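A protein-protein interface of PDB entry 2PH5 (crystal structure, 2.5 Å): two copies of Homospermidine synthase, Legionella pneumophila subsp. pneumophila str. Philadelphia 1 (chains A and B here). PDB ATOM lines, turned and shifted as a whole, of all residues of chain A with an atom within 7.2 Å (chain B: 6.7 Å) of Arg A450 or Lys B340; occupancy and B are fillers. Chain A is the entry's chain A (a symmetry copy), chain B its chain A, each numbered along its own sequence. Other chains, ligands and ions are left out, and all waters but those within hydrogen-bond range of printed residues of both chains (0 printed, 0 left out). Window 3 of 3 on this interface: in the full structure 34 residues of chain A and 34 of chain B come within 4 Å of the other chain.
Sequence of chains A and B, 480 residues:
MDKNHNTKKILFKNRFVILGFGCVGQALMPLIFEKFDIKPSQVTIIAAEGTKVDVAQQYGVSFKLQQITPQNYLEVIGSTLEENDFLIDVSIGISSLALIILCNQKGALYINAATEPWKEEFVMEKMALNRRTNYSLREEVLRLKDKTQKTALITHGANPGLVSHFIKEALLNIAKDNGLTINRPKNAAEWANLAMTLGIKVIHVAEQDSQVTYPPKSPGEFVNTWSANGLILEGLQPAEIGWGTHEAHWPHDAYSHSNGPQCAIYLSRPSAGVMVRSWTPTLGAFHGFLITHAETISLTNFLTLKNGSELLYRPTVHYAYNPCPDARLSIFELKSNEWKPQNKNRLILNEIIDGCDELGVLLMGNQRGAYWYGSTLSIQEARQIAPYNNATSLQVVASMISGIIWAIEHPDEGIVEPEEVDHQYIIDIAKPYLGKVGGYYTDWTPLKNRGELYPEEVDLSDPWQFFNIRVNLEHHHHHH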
ATOM      1  N   ARG A 277      15.198 -17.792  16.155  1.00  0.00           N
ATOM      2  CA  ARG A 277      15.141 -17.894  14.704  1.00  0.00           C
ATOM      3  C   ARG A 277      15.962 -19.094  14.230  1.00  0.00           C
ATOM      4  O   ARG A 277      17.166 -19.143  14.449  1.00  0.00           O
ATOM      5  CB  ARG A 277      15.710 -16.620  14.070  1.00  0.00           C
ATOM      6  CG  ARG A 277      14.910 -15.354  14.351  1.00  0.00           C
ATOM      7  CD  ARG A 277      15.535 -14.118  13.705  1.00  0.00           C
ATOM      8  NE  ARG A 277      14.664 -12.953  13.841  1.00  0.00           N
ATOM      9  CZ  ARG A 277      14.655 -12.126  14.884  1.00  0.00           C
ATOM     10  NH1 ARG A 277      15.486 -12.319  15.901  1.00  0.00           N
ATOM     11  NH2 ARG A 277      13.791 -11.121  14.927  1.00  0.00           N
ATOM     12  N   HIS A 287      10.140 -19.354  13.584  1.00  0.00           N
ATOM     13  CA  HIS A 287      10.431 -18.974  14.959  1.00  0.00           C
ATOM     14  C   HIS A 287      10.021 -20.113  15.880  1.00  0.00           C
ATOM     15  O   HIS A 287       8.833 -20.358  16.091  1.00  0.00           O
ATOM     16  CB  HIS A 287       9.681 -17.705  15.368  1.00  0.00           C
ATOM     17  CG  HIS A 287      10.224 -16.451  14.754  1.00  0.00           C
ATOM     18  ND1 HIS A 287       9.857 -15.193  15.186  1.00  0.00           N
ATOM     19  CD2 HIS A 287      11.087 -16.262  13.727  1.00  0.00           C
ATOM     20  CE1 HIS A 287      10.473 -14.284  14.450  1.00  0.00           C
ATOM     21  NE2 HIS A 287      11.224 -14.905  13.558  1.00  0.00           N
ATOM     22  N   THR A 445      20.100 -16.974   6.954  1.00  0.00           N
ATOM     23  CA  THR A 445      20.755 -16.538   8.182  1.00  0.00           C
ATOM     24  C   THR A 445      19.691 -15.734   8.911  1.00  0.00           C
ATOM     25  O   THR A 445      18.751 -15.250   8.294  1.00  0.00           O
ATOM     26  CB  THR A 445      21.974 -15.611   7.958  1.00  0.00           C
ATOM     27  OG1 THR A 445      21.542 -14.246   7.983  1.00  0.00           O
ATOM     28  CG2 THR A 445      22.644 -15.906   6.630  1.00  0.00           C
ATOM     29  N   PRO A 446      19.815 -15.589  10.239  1.00  0.00           N
ATOM     30  CA  PRO A 446      18.810 -14.818  10.984  1.00  0.00           C
ATOM     31  C   PRO A 446      18.875 -13.331  10.675  1.00  0.00           C
ATOM     32  O   PRO A 446      18.149 -12.533  11.263  1.00  0.00           O
ATOM     33  CB  PRO A 446      19.149 -15.122  12.441  1.00  0.00           C
ATOM     34  CG  PRO A 446      20.618 -15.347  12.406  1.00  0.00           C
ATOM     35  CD  PRO A 446      20.808 -16.185  11.152  1.00  0.00           C
ATOM     36  N   LEU A 447      19.742 -12.973   9.736  1.00  0.00           N
ATOM     37  CA  LEU A 447      19.925 -11.576   9.360  1.00  0.00           C
ATOM     38  C   LEU A 447      19.158 -11.155   8.107  1.00  0.00           C
ATOM     39  O   LEU A 447      18.919  -9.966   7.895  1.00  0.00           O
ATOM     40  CB  LEU A 447      21.415 -11.283   9.182  1.00  0.00           C
ATOM     41  CG  LEU A 447      22.043 -10.263  10.130  1.00  0.00           C
ATOM     42  CD1 LEU A 447      21.588 -10.493  11.554  1.00  0.00           C
ATOM     43  CD2 LEU A 447      23.564 -10.369  10.029  1.00  0.00           C
ATOM     44  N   LYS A 448      18.768 -12.112   7.275  1.00  0.00           N
ATOM     45  CA  LYS A 448      18.039 -11.763   6.068  1.00  0.00           C
ATOM     46  C   LYS A 448      16.539 -11.982   6.180  1.00  0.00           C
ATOM     47  O   LYS A 448      16.057 -12.559   7.156  1.00  0.00           O
ATOM     48  CB  LYS A 448      18.603 -12.521   4.863  1.00  0.00           C
ATOM     49  CG  LYS A 448      18.805 -13.993   5.081  1.00  0.00           C
ATOM     50  CD  LYS A 448      20.136 -14.419   4.479  1.00  0.00           C
ATOM     51  CE  LYS A 448      20.253 -14.018   3.016  1.00  0.00           C
ATOM     52  NZ  LYS A 448      21.631 -14.275   2.507  1.00  0.00           N
ATOM     53  N   ASN A 449      15.812 -11.505   5.170  1.00  0.00           N
ATOM     54  CA  ASN A 449      14.353 -11.592   5.112  1.00  0.00           C
ATOM     55  C   ASN A 449      13.761 -10.856   6.301  1.00  0.00           C
ATOM     56  O   ASN A 449      12.586 -11.019   6.631  1.00  0.00           O
ATOM     57  CB  ASN A 449      13.880 -13.044   5.118  1.00  0.00           C
ATOM     58  CG  ASN A 449      14.402 -13.827   3.936  1.00  0.00           C
ATOM     59  OD1 ASN A 449      14.257 -13.408   2.785  1.00  0.00           O
ATOM     60  ND2 ASN A 449      15.011 -14.980   4.211  1.00  0.00           N
ATOM     61  N   ARG A 450      14.597 -10.045   6.942  1.00  0.00           N
ATOM     62  CA  ARG A 450      14.187  -9.260   8.093  1.00  0.00           C
ATOM     63  C   ARG A 450      13.121  -8.259   7.706  1.00  0.00           C
ATOM     64  O   ARG A 450      13.019  -7.853   6.546  1.00  0.00           O
ATOM     65  CB  ARG A 450      15.386  -8.511   8.674  1.00  0.00           C
ATOM     66  CG  ARG A 450      16.303  -9.357   9.542  1.00  0.00           C
ATOM     67  CD  ARG A 450      15.721  -9.541  10.926  1.00  0.00           C
ATOM     68  NE  ARG A 450      16.734 -10.003  11.863  1.00  0.00           N
ATOM     69  CZ  ARG A 450      16.633  -9.889  13.181  1.00  0.00           C
ATOM     70  NH1 ARG A 450      17.598 -10.333  13.967  1.00  0.00           N
ATOM     71  NH2 ARG A 450      15.569  -9.321  13.720  1.00  0.00           N
ATOM     72  N   GLY A 451      12.330  -7.852   8.689  1.00  0.00           N
ATOM     73  CA  GLY A 451      11.284  -6.884   8.432  1.00  0.00           C
ATOM     74  C   GLY A 451      11.791  -5.481   8.685  1.00  0.00           C
ATOM     75  O   GLY A 451      12.946  -5.282   9.075  1.00  0.00           O
ATOM     76  N   GLU A 452      10.925  -4.502   8.456  1.00  0.00           N
ATOM     77  CA  GLU A 452      11.296  -3.116   8.677  1.00  0.00           C
ATOM     78  C   GLU A 452      10.236  -2.358   9.466  1.00  0.00           C
ATOM     79  O   GLU A 452      10.450  -1.204   9.842  1.00  0.00           O
ATOM     80  CB  GLU A 452      11.550  -2.421   7.338  1.00  0.00           C
ATOM     81  CG  GLU A 452      10.370  -2.451   6.392  1.00  0.00           C
ATOM     82  CD  GLU A 452      10.684  -1.813   5.057  1.00  0.00           C
ATOM     83  OE1 GLU A 452       9.781  -1.781   4.192  1.00  0.00           O
ATOM     84  OE2 GLU A 452      11.831  -1.345   4.873  1.00  0.00           O
ATOM     85  N   LEU A 453       9.099  -3.005   9.723  1.00  0.00           N
ATOM     86  CA  LEU A 453       8.027  -2.367  10.487  1.00  0.00           C
ATOM     87  C   LEU A 453       8.574  -1.956  11.854  1.00  0.00           C
ATOM     88  O   LEU A 453       8.363  -0.829  12.315  1.00  0.00           O
ATOM     89  CB  LEU A 453       6.834  -3.319  10.662  1.00  0.00           C
ATOM     90  CG  LEU A 453       5.980  -3.687   9.437  1.00  0.00           C
ATOM     91  CD1 LEU A 453       5.455  -2.419   8.781  1.00  0.00           C
ATOM     92  CD2 LEU A 453       6.798  -4.506   8.449  1.00  0.00           C
ATOM     93  N   TYR A 454       9.280  -2.880  12.501  1.00  0.00           N
ATOM     94  CA  TYR A 454       9.884  -2.612  13.800  1.00  0.00           C
ATOM     95  C   TYR A 454      11.326  -3.123  13.794  1.00  0.00           C
ATOM     96  O   TYR A 454      11.589  -4.288  14.096  1.00  0.00           O
ATOM     97  CB  TYR A 454       9.066  -3.270  14.921  1.00  0.00           C
ATOM     98  CG  TYR A 454       7.708  -2.620  15.128  1.00  0.00           C
ATOM     99  CD1 TYR A 454       6.667  -2.823  14.220  1.00  0.00           C
ATOM    100  CD2 TYR A 454       7.482  -1.750  16.200  1.00  0.00           C
ATOM    101  CE1 TYR A 454       5.438  -2.175  14.367  1.00  0.00           C
ATOM    102  CE2 TYR A 454       6.252  -1.096  16.357  1.00  0.00           C
ATOM    103  CZ  TYR A 454       5.238  -1.313  15.435  1.00  0.00           C
ATOM    104  OH  TYR A 454       4.030  -0.671  15.568  1.00  0.00           O
ATOM    105  N   PRO A 455      12.283  -2.242  13.444  1.00  0.00           N
ATOM    106  CA  PRO A 455      13.709  -2.588  13.385  1.00  0.00           C
ATOM    107  C   PRO A 455      14.287  -3.108  14.700  1.00  0.00           C
ATOM    108  O   PRO A 455      14.385  -2.366  15.683  1.00  0.00           O
ATOM    109  CB  PRO A 455      14.363  -1.278  12.945  1.00  0.00           C
ATOM    110  CG  PRO A 455      13.481  -0.247  13.568  1.00  0.00           C
ATOM    111  CD  PRO A 455      12.097  -0.790  13.258  1.00  0.00           C
ATOM    112  N   GLU A 456      14.665  -4.384  14.706  1.00  0.00           N
ATOM    113  CA  GLU A 456      15.256  -5.014  15.885  1.00  0.00           C
ATOM    114  C   GLU A 456      16.775  -4.902  15.784  1.00  0.00           C
ATOM    115  O   GLU A 456      17.359  -5.254  14.764  1.00  0.00           O
ATOM    116  CB  GLU A 456      14.836  -6.490  15.977  1.00  0.00           C
ATOM    117  CG  GLU A 456      15.522  -7.269  17.098  1.00  0.00           C
ATOM    118  CD  GLU A 456      14.930  -8.667  17.319  1.00  0.00           C
ATOM    119  OE1 GLU A 456      15.523  -9.448  18.104  1.00  0.00           O
ATOM    120  OE2 GLU A 456      13.876  -8.983  16.721  1.00  0.00           O
ATOM    121  N   GLU A 457      17.411  -4.396  16.835  1.00  0.00           N
ATOM    122  CA  GLU A 457      18.861  -4.234  16.844  1.00  0.00           C
ATOM    123  C   GLU A 457      19.550  -5.548  16.481  1.00  0.00           C
ATOM    124  O   GLU A 457      19.302  -6.582  17.091  1.00  0.00           O
ATOM    125  CB  GLU A 457      19.316  -3.758  18.225  1.00  0.00           C
ATOM    126  CG  GLU A 457      20.665  -3.062  18.245  1.00  0.00           C
ATOM    127  CD  GLU A 457      20.967  -2.447  19.599  1.00  0.00           C
ATOM    128  OE1 GLU A 457      20.130  -1.664  20.093  1.00  0.00           O
ATOM    129  OE2 GLU A 457      22.042  -2.742  20.166  1.00  0.00           O
ATOM    130  N   VAL A 458      20.410  -5.499  15.472  1.00  0.00           N
ATOM    131  CA  VAL A 458      21.115  -6.691  15.035  1.00  0.00           C
ATOM    132  C   VAL A 458      22.610  -6.447  14.938  1.00  0.00           C
ATOM    133  O   VAL A 458      23.066  -5.310  14.931  1.00  0.00           O
ATOM    134  CB  VAL A 458      20.610  -7.156  13.662  1.00  0.00           C
ATOM    135  CG1 VAL A 458      19.145  -7.564  13.755  1.00  0.00           C
ATOM    136  CG2 VAL A 458      20.790  -6.041  12.650  1.00  0.00           C
ATOM    137  N   ASP A 459      23.369  -7.529  14.857  1.00  0.00           N
ATOM    138  CA  ASP A 459      24.820  -7.456  14.751  1.00  0.00           C
ATOM    139  C   ASP A 459      25.201  -7.976  13.357  1.00  0.00           C
ATOM    140  O   ASP A 459      25.354  -9.184  13.146  1.00  0.00           O
ATOM    141  CB  ASP A 459      25.444  -8.317  15.856  1.00  0.00           C
ATOM    142  CG  ASP A 459      26.955  -8.216  15.908  1.00  0.00           C
ATOM    143  OD1 ASP A 459      27.551  -8.782  16.853  1.00  0.00           O
ATOM    144  OD2 ASP A 459      27.552  -7.582  15.012  1.00  0.00           O
ATOM    145  N   PHE A 467      22.543 -12.828  19.783  1.00  0.00           N
ATOM    146  CA  PHE A 467      21.923 -11.508  19.788  1.00  0.00           C
ATOM    147  C   PHE A 467      20.969 -11.354  18.584  1.00  0.00           C
ATOM    148  O   PHE A 467      19.948 -10.670  18.683  1.00  0.00           O
ATOM    149  CB  PHE A 467      23.030 -10.446  19.739  1.00  0.00           C
ATOM    150  CG  PHE A 467      22.559  -9.046  20.003  1.00  0.00           C
ATOM    151  CD1 PHE A 467      22.166  -8.651  21.274  1.00  0.00           C
ATOM    152  CD2 PHE A 467      22.548  -8.110  18.980  1.00  0.00           C
ATOM    153  CE1 PHE A 467      21.773  -7.337  21.523  1.00  0.00           C
ATOM    154  CE2 PHE A 467      22.158  -6.794  19.215  1.00  0.00           C
ATOM    155  CZ  PHE A 467      21.769  -6.405  20.489  1.00  0.00           C
ATOM    156  N   ASN A 468      21.298 -11.992  17.457  1.00  0.00           N
ATOM    157  CA  ASN A 468      20.459 -11.914  16.253  1.00  0.00           C
ATOM    158  C   ASN A 468      19.396 -13.011  16.186  1.00  0.00           C
ATOM    159  O   ASN A 468      18.329 -12.820  15.600  1.00  0.00           O
ATOM    160  CB  ASN A 468      21.299 -12.016  14.971  1.00  0.00           C
ATOM    161  CG  ASN A 468      22.322 -10.911  14.843  1.00  0.00           C
ATOM    162  OD1 ASN A 468      22.000  -9.722  14.952  1.00  0.00           O
ATOM    163  ND2 ASN A 468      23.570 -11.295  14.589  1.00  0.00           N
ATOM    164  N   ILE A 469      19.694 -14.162  16.776  1.00  0.00           N
ATOM    165  CA  ILE A 469      18.773 -15.288  16.743  1.00  0.00           C
ATOM    166  C   ILE A 469      17.588 -15.137  17.698  1.00  0.00           C
ATOM    167  O   ILE A 469      16.444 -15.389  17.314  1.00  0.00           O
ATOM    168  CB  ILE A 469      19.539 -16.603  17.006  1.00  0.00           C
ATOM    169  CG1 ILE A 469      20.516 -16.836  15.841  1.00  0.00           C
ATOM    170  CG2 ILE A 469      18.563 -17.777  17.138  1.00  0.00           C
ATOM    171  CD1 ILE A 469      21.631 -17.820  16.125  1.00  0.00           C
ATOM    172  N   ARG A 470      17.845 -14.706  18.926  1.00  0.00           N
ATOM    173  CA  ARG A 470      16.752 -14.529  19.862  1.00  0.00           C
ATOM    174  C   ARG A 470      15.829 -13.395  19.431  1.00  0.00           C
ATOM    175  O   ARG A 470      16.269 -12.267  19.222  1.00  0.00           O
ATOM    176  CB  ARG A 470      17.257 -14.223  21.263  1.00  0.00           C
ATOM    177  CG  ARG A 470      16.114 -14.145  22.248  1.00  0.00           C
ATOM    178  CD  ARG A 470      16.532 -13.469  23.493  1.00  0.00           C
ATOM    179  NE  ARG A 470      15.451 -13.384  24.460  1.00  0.00           N
ATOM    180  CZ  ARG A 470      15.646 -13.067  25.732  1.00  0.00           C
ATOM    181  NH1 ARG A 470      14.623 -13.000  26.578  1.00  0.00           N
ATOM    182  NH2 ARG A 470      16.878 -12.826  26.161  1.00  0.00           N
ATOM    183  N   VAL A 471      14.545 -13.709  19.316  1.00  0.00           N
ATOM    184  CA  VAL A 471      13.543 -12.738  18.916  1.00  0.00           C
ATOM    185  C   VAL A 471      13.247 -11.804  20.080  1.00  0.00           C
ATOM    186  O   VAL A 471      12.413 -12.104  20.928  1.00  0.00           O
ATOM    187  CB  VAL A 471      12.253 -13.454  18.474  1.00  0.00           C
ATOM    188  CG1 VAL A 471      11.182 -12.443  18.091  1.00  0.00           C
ATOM    189  CG2 VAL A 471      12.565 -14.372  17.306  1.00  0.00           C
ATOM    190  N   ASN A 472      13.947 -10.676  20.125  1.00  0.00           N
ATOM    191  CA  ASN A 472      13.753  -9.705  21.191  1.00  0.00           C
ATOM    192  C   ASN A 472      12.582  -8.782  20.896  1.00  0.00           C
ATOM    193  O   ASN A 472      12.551  -8.092  19.874  1.00  0.00           O
ATOM    194  CB  ASN A 472      15.019  -8.867  21.409  1.00  0.00           C
ATOM    195  CG  ASN A 472      16.048  -9.563  22.299  1.00  0.00           C
ATOM    196  OD1 ASN A 472      16.611 -10.599  21.931  1.00  0.00           O
ATOM    197  ND2 ASN A 472      16.302  -8.988  23.473  1.00  0.00           N
ATOM    198  N   LEU B 236      -0.457  -4.722  13.088  1.00  0.00           N
ATOM    199  CA  LEU B 236       0.838  -4.136  12.764  1.00  0.00           C
ATOM    200  C   LEU B 236       1.033  -2.769  13.417  1.00  0.00           C
ATOM    201  O   LEU B 236       2.156  -2.387  13.734  1.00  0.00           O
ATOM    202  CB  LEU B 236       0.999  -4.017  11.243  1.00  0.00           C
ATOM    203  CG  LEU B 236       2.025  -4.930  10.550  1.00  0.00           C
ATOM    204  CD1 LEU B 236       1.789  -6.376  10.912  1.00  0.00           C
ATOM    205  CD2 LEU B 236       1.936  -4.734   9.037  1.00  0.00           C
ATOM    206  N   GLU B 333       2.326 -17.279  12.754  1.00  0.00           N
ATOM    207  CA  GLU B 333       3.106 -17.450  11.530  1.00  0.00           C
ATOM    208  C   GLU B 333       3.573 -16.100  10.967  1.00  0.00           C
ATOM    209  O   GLU B 333       4.659 -16.008  10.391  1.00  0.00           O
ATOM    210  CB  GLU B 333       2.267 -18.217  10.494  1.00  0.00           C
ATOM    211  CG  GLU B 333       2.870 -18.340   9.101  1.00  0.00           C
ATOM    212  CD  GLU B 333       2.009 -19.191   8.161  1.00  0.00           C
ATOM    213  OE1 GLU B 333       0.792 -18.917   8.040  1.00  0.00           O
ATOM    214  OE2 GLU B 333       2.550 -20.138   7.536  1.00  0.00           O
ATOM    215  N   LEU B 334       2.753 -15.064  11.155  1.00  0.00           N
ATOM    216  CA  LEU B 334       3.039 -13.698  10.699  1.00  0.00           C
ATOM    217  C   LEU B 334       4.303 -13.198  11.388  1.00  0.00           C
ATOM    218  O   LEU B 334       5.241 -12.744  10.735  1.00  0.00           O
ATOM    219  CB  LEU B 334       1.876 -12.769  11.064  1.00  0.00           C
ATOM    220  CG  LEU B 334       1.634 -11.425  10.355  1.00  0.00           C
ATOM    221  CD1 LEU B 334       1.232 -10.401  11.411  1.00  0.00           C
ATOM    222  CD2 LEU B 334       2.842 -10.950   9.579  1.00  0.00           C
ATOM    223  N   LYS B 335       4.315 -13.281  12.717  1.00  0.00           N
ATOM    224  CA  LYS B 335       5.467 -12.856  13.508  1.00  0.00           C
ATOM    225  C   LYS B 335       6.656 -13.725  13.123  1.00  0.00           C
ATOM    226  O   LYS B 335       7.778 -13.234  12.999  1.00  0.00           O
ATOM    227  CB  LYS B 335       5.194 -13.025  15.007  1.00  0.00           C
ATOM    228  CG  LYS B 335       4.072 -12.171  15.547  1.00  0.00           C
ATOM    229  CD  LYS B 335       3.745 -12.544  16.975  1.00  0.00           C
ATOM    230  CE  LYS B 335       2.659 -11.628  17.506  1.00  0.00           C
ATOM    231  NZ  LYS B 335       2.238 -11.938  18.905  1.00  0.00           N
ATOM    232  N   SER B 336       6.394 -15.019  12.949  1.00  0.00           N
ATOM    233  CA  SER B 336       7.414 -15.987  12.562  1.00  0.00           C
ATOM    234  C   SER B 336       8.069 -15.575  11.240  1.00  0.00           C
ATOM    235  O   SER B 336       9.245 -15.852  11.009  1.00  0.00           O
ATOM    236  CB  SER B 336       6.786 -17.378  12.424  1.00  0.00           C
ATOM    237  OG  SER B 336       7.728 -18.343  11.988  1.00  0.00           O
ATOM    238  N   ASN B 337       7.299 -14.913  10.376  1.00  0.00           N
ATOM    239  CA  ASN B 337       7.805 -14.449   9.089  1.00  0.00           C
ATOM    240  C   ASN B 337       8.292 -13.014   9.204  1.00  0.00           C
ATOM    241  O   ASN B 337       8.228 -12.251   8.236  1.00  0.00           O
ATOM    242  CB  ASN B 337       6.724 -14.486   8.006  1.00  0.00           C
ATOM    243  CG  ASN B 337       6.161 -15.864   7.774  1.00  0.00           C
ATOM    244  OD1 ASN B 337       6.879 -16.867   7.807  1.00  0.00           O
ATOM    245  ND2 ASN B 337       4.862 -15.924   7.511  1.00  0.00           N
ATOM    246  N   GLU B 338       8.759 -12.640  10.389  1.00  0.00           N
ATOM    247  CA  GLU B 338       9.264 -11.290  10.608  1.00  0.00           C
ATOM    248  C   GLU B 338       8.272 -10.184  10.183  1.00  0.00           C
ATOM    249  O   GLU B 338       8.662  -9.196   9.555  1.00  0.00           O
ATOM    250  CB  GLU B 338      10.593 -11.131   9.860  1.00  0.00           C
ATOM    251  CG  GLU B 338      11.811 -10.905  10.758  1.00  0.00           C
ATOM    252  CD  GLU B 338      12.229 -12.123  11.577  1.00  0.00           C
ATOM    253  OE1 GLU B 338      12.754 -11.914  12.684  1.00  0.00           O
ATOM    254  OE2 GLU B 338      12.064 -13.273  11.123  1.00  0.00           O
ATOM    255  N   TRP B 339       6.992 -10.360  10.527  1.00  0.00           N
ATOM    256  CA  TRP B 339       5.929  -9.395  10.204  1.00  0.00           C
ATOM    257  C   TRP B 339       5.591  -9.292   8.716  1.00  0.00           C
ATOM    258  O   TRP B 339       4.845  -8.405   8.296  1.00  0.00           O
ATOM    259  CB  TRP B 339       6.283  -8.004  10.750  1.00  0.00           C
ATOM    260  CG  TRP B 339       6.373  -7.961  12.247  1.00  0.00           C
ATOM    261  CD1 TRP B 339       7.481  -7.684  12.993  1.00  0.00           C
ATOM    262  CD2 TRP B 339       5.325  -8.243  13.180  1.00  0.00           C
ATOM    263  NE1 TRP B 339       7.190  -7.780  14.331  1.00  0.00           N
ATOM    264  CE2 TRP B 339       5.873  -8.122  14.477  1.00  0.00           C
ATOM    265  CE3 TRP B 339       3.974  -8.587  13.046  1.00  0.00           C
ATOM    266  CZ2 TRP B 339       5.118  -8.334  15.637  1.00  0.00           C
ATOM    267  CZ3 TRP B 339       3.220  -8.799  14.202  1.00  0.00           C
ATOM    268  CH2 TRP B 339       3.797  -8.670  15.479  1.00  0.00           C
ATOM    269  N   LYS B 340       6.151 -10.204   7.927  1.00  0.00           N
ATOM    270  CA  LYS B 340       5.905 -10.269   6.491  1.00  0.00           C
ATOM    271  C   LYS B 340       4.609 -11.051   6.319  1.00  0.00           C
ATOM    272  O   LYS B 340       4.564 -12.249   6.602  1.00  0.00           O
ATOM    273  CB  LYS B 340       7.010 -11.056   5.786  1.00  0.00           C
ATOM    274  CG  LYS B 340       7.886 -10.279   4.839  1.00  0.00           C
ATOM    275  CD  LYS B 340       8.928  -9.482   5.597  1.00  0.00           C
ATOM    276  CE  LYS B 340      10.220  -9.399   4.786  1.00  0.00           C
ATOM    277  NZ  LYS B 340       9.957  -8.971   3.380  1.00  0.00           N
ATOM    278  N   PRO B 341       3.543 -10.393   5.850  1.00  0.00           N
ATOM    279  CA  PRO B 341       2.272 -11.094   5.662  1.00  0.00           C
ATOM    280  C   PRO B 341       2.357 -12.242   4.658  1.00  0.00           C
ATOM    281  O   PRO B 341       3.060 -12.153   3.650  1.00  0.00           O
ATOM    282  CB  PRO B 341       1.322  -9.979   5.219  1.00  0.00           C
ATOM    283  CG  PRO B 341       2.236  -8.982   4.574  1.00  0.00           C
ATOM    284  CD  PRO B 341       3.419  -8.970   5.500  1.00  0.00           C
ATOM    285  N   GLN B 342       1.649 -13.325   4.965  1.00  0.00           N
ATOM    286  CA  GLN B 342       1.614 -14.511   4.115  1.00  0.00           C
ATOM    287  C   GLN B 342       1.209 -14.099   2.705  1.00  0.00           C
ATOM    288  O   GLN B 342       0.441 -13.157   2.525  1.00  0.00           O
ATOM    289  CB  GLN B 342       0.593 -15.522   4.651  1.00  0.00           C
ATOM    290  CG  GLN B 342       0.933 -16.196   5.978  1.00  0.00           C
ATOM    291  CD  GLN B 342       0.338 -15.499   7.195  1.00  0.00           C
ATOM    292  OE1 GLN B 342      -0.023 -16.154   8.176  1.00  0.00           O
ATOM    293  NE2 GLN B 342       0.245 -14.173   7.143  1.00  0.00           N
ATOM    294  N   ASN B 343       1.715 -14.809   1.704  1.00  0.00           N
ATOM    295  CA  ASN B 343       1.378 -14.482   0.324  1.00  0.00           C
ATOM    296  C   ASN B 343      -0.056 -14.887  -0.027  1.00  0.00           C
ATOM    297  O   ASN B 343      -0.551 -14.566  -1.112  1.00  0.00           O
ATOM    298  CB  ASN B 343       2.365 -15.153  -0.640  1.00  0.00           C
ATOM    299  CG  ASN B 343       3.784 -14.635  -0.470  1.00  0.00           C
ATOM    300  OD1 ASN B 343       3.997 -13.435  -0.265  1.00  0.00           O
ATOM    301  ND2 ASN B 343       4.763 -15.531  -0.569  1.00  0.00           N
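O of Leu B236 is in hydrogen-bond range of OH of Tyr A454, at 3.1 Å. OG of Ser B336 sits at hydrogen-bond distance from N of His A287 (3.1 Å). OE1 of Glu B338 lies within salt-bridge range of NE of Arg A277 (2.5 Å). OE2 of Glu B338 lies within hydrogen-bond range of NE2 of His A287 (3.0 Å). OE1 of Glu B338 lies within salt-bridge range of NH2 of Arg A450 (3.96 Å).
The side-chain carboxylate (OE2) of Glu A456 lies within salt-bridge range of the guanidinium group (NH2) of Arg A277, at 2.8 Å. O of Asn A468 lies within hydrogen-bond range of NH1 of Arg A277, at 2.9 Å. NH1 of Arg A277 is in hydrogen-bond range of O of Arg A470 (3.4 Å). The guanidinium group of Arg A450 is in hydrogen-bond range of the backbone carbonyl oxygen of Pro A446. The side-chain carboxylate (OE2) of Glu A456 is in salt-bridge range of the guanidinium group (NH2) of Arg A450. The backbone carbonyl oxygen (O) of Asn A468 sits at hydrogen-bond distance from the guanidinium group (NH1) of Arg A450 (3.1 Å).
O of Lys B335 touches CE1 of His A287, 3.2 Å away. Glu B338 touches Asn A449 (CB to O, 3.8 Å). Lys B340 touches Asn A449 (CE to O, 3.4 Å). O of Arg A450 touches CE of Lys B340 (3.6 Å). Gly A451 touches Glu B338.
Of the printed residues of chain B, Arg A450 touches Glu B338 (3.9 Å) and Lys B340 (3.6 Å). Lys B340 touches just these residues of chain A: Asn A449 (3.4 Å) and Arg A450 (3.6 Å). Printed residues of chain B within 4 Å of Arg A277: Glu B338 (2.5 Å). Printed residues of chain B within 4 Å of Tyr A454: Leu B236. Printed residues of chain A within 4 Å of Glu B338: Arg A277 (2.5 Å), His A287 (3.0 Å), Asn A449 (3.8 Å), Arg A450 (3.9 Å) and Gly A451 (3.7 Å). Of the printed residues of chain B, His A287 touches Lys B335, Ser B336 and Glu B338. Leu A453 touches none of the printed residues of chain B.
Of the 23 printed residues of chain A, 6 touch a printed residue of chain B. Hydrophobic or aromatic side chains of chain A within 4 Å of the printed part of chain B: His A287 and Tyr A454. Of the 12 printed residues of chain B, 5 touch a printed residue of chain A. Among the printed residues, 10 pairs touch across the chains. Among the printed residues, Asp or Glu carboxylates within 4 Å of a Lys or Arg side-chain nitrogen of the other chain: Arg A277 with Glu B338 (2.5 Å) and Arg A450 with Glu B338 (3.96 Å).
No position is printed for both chains.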
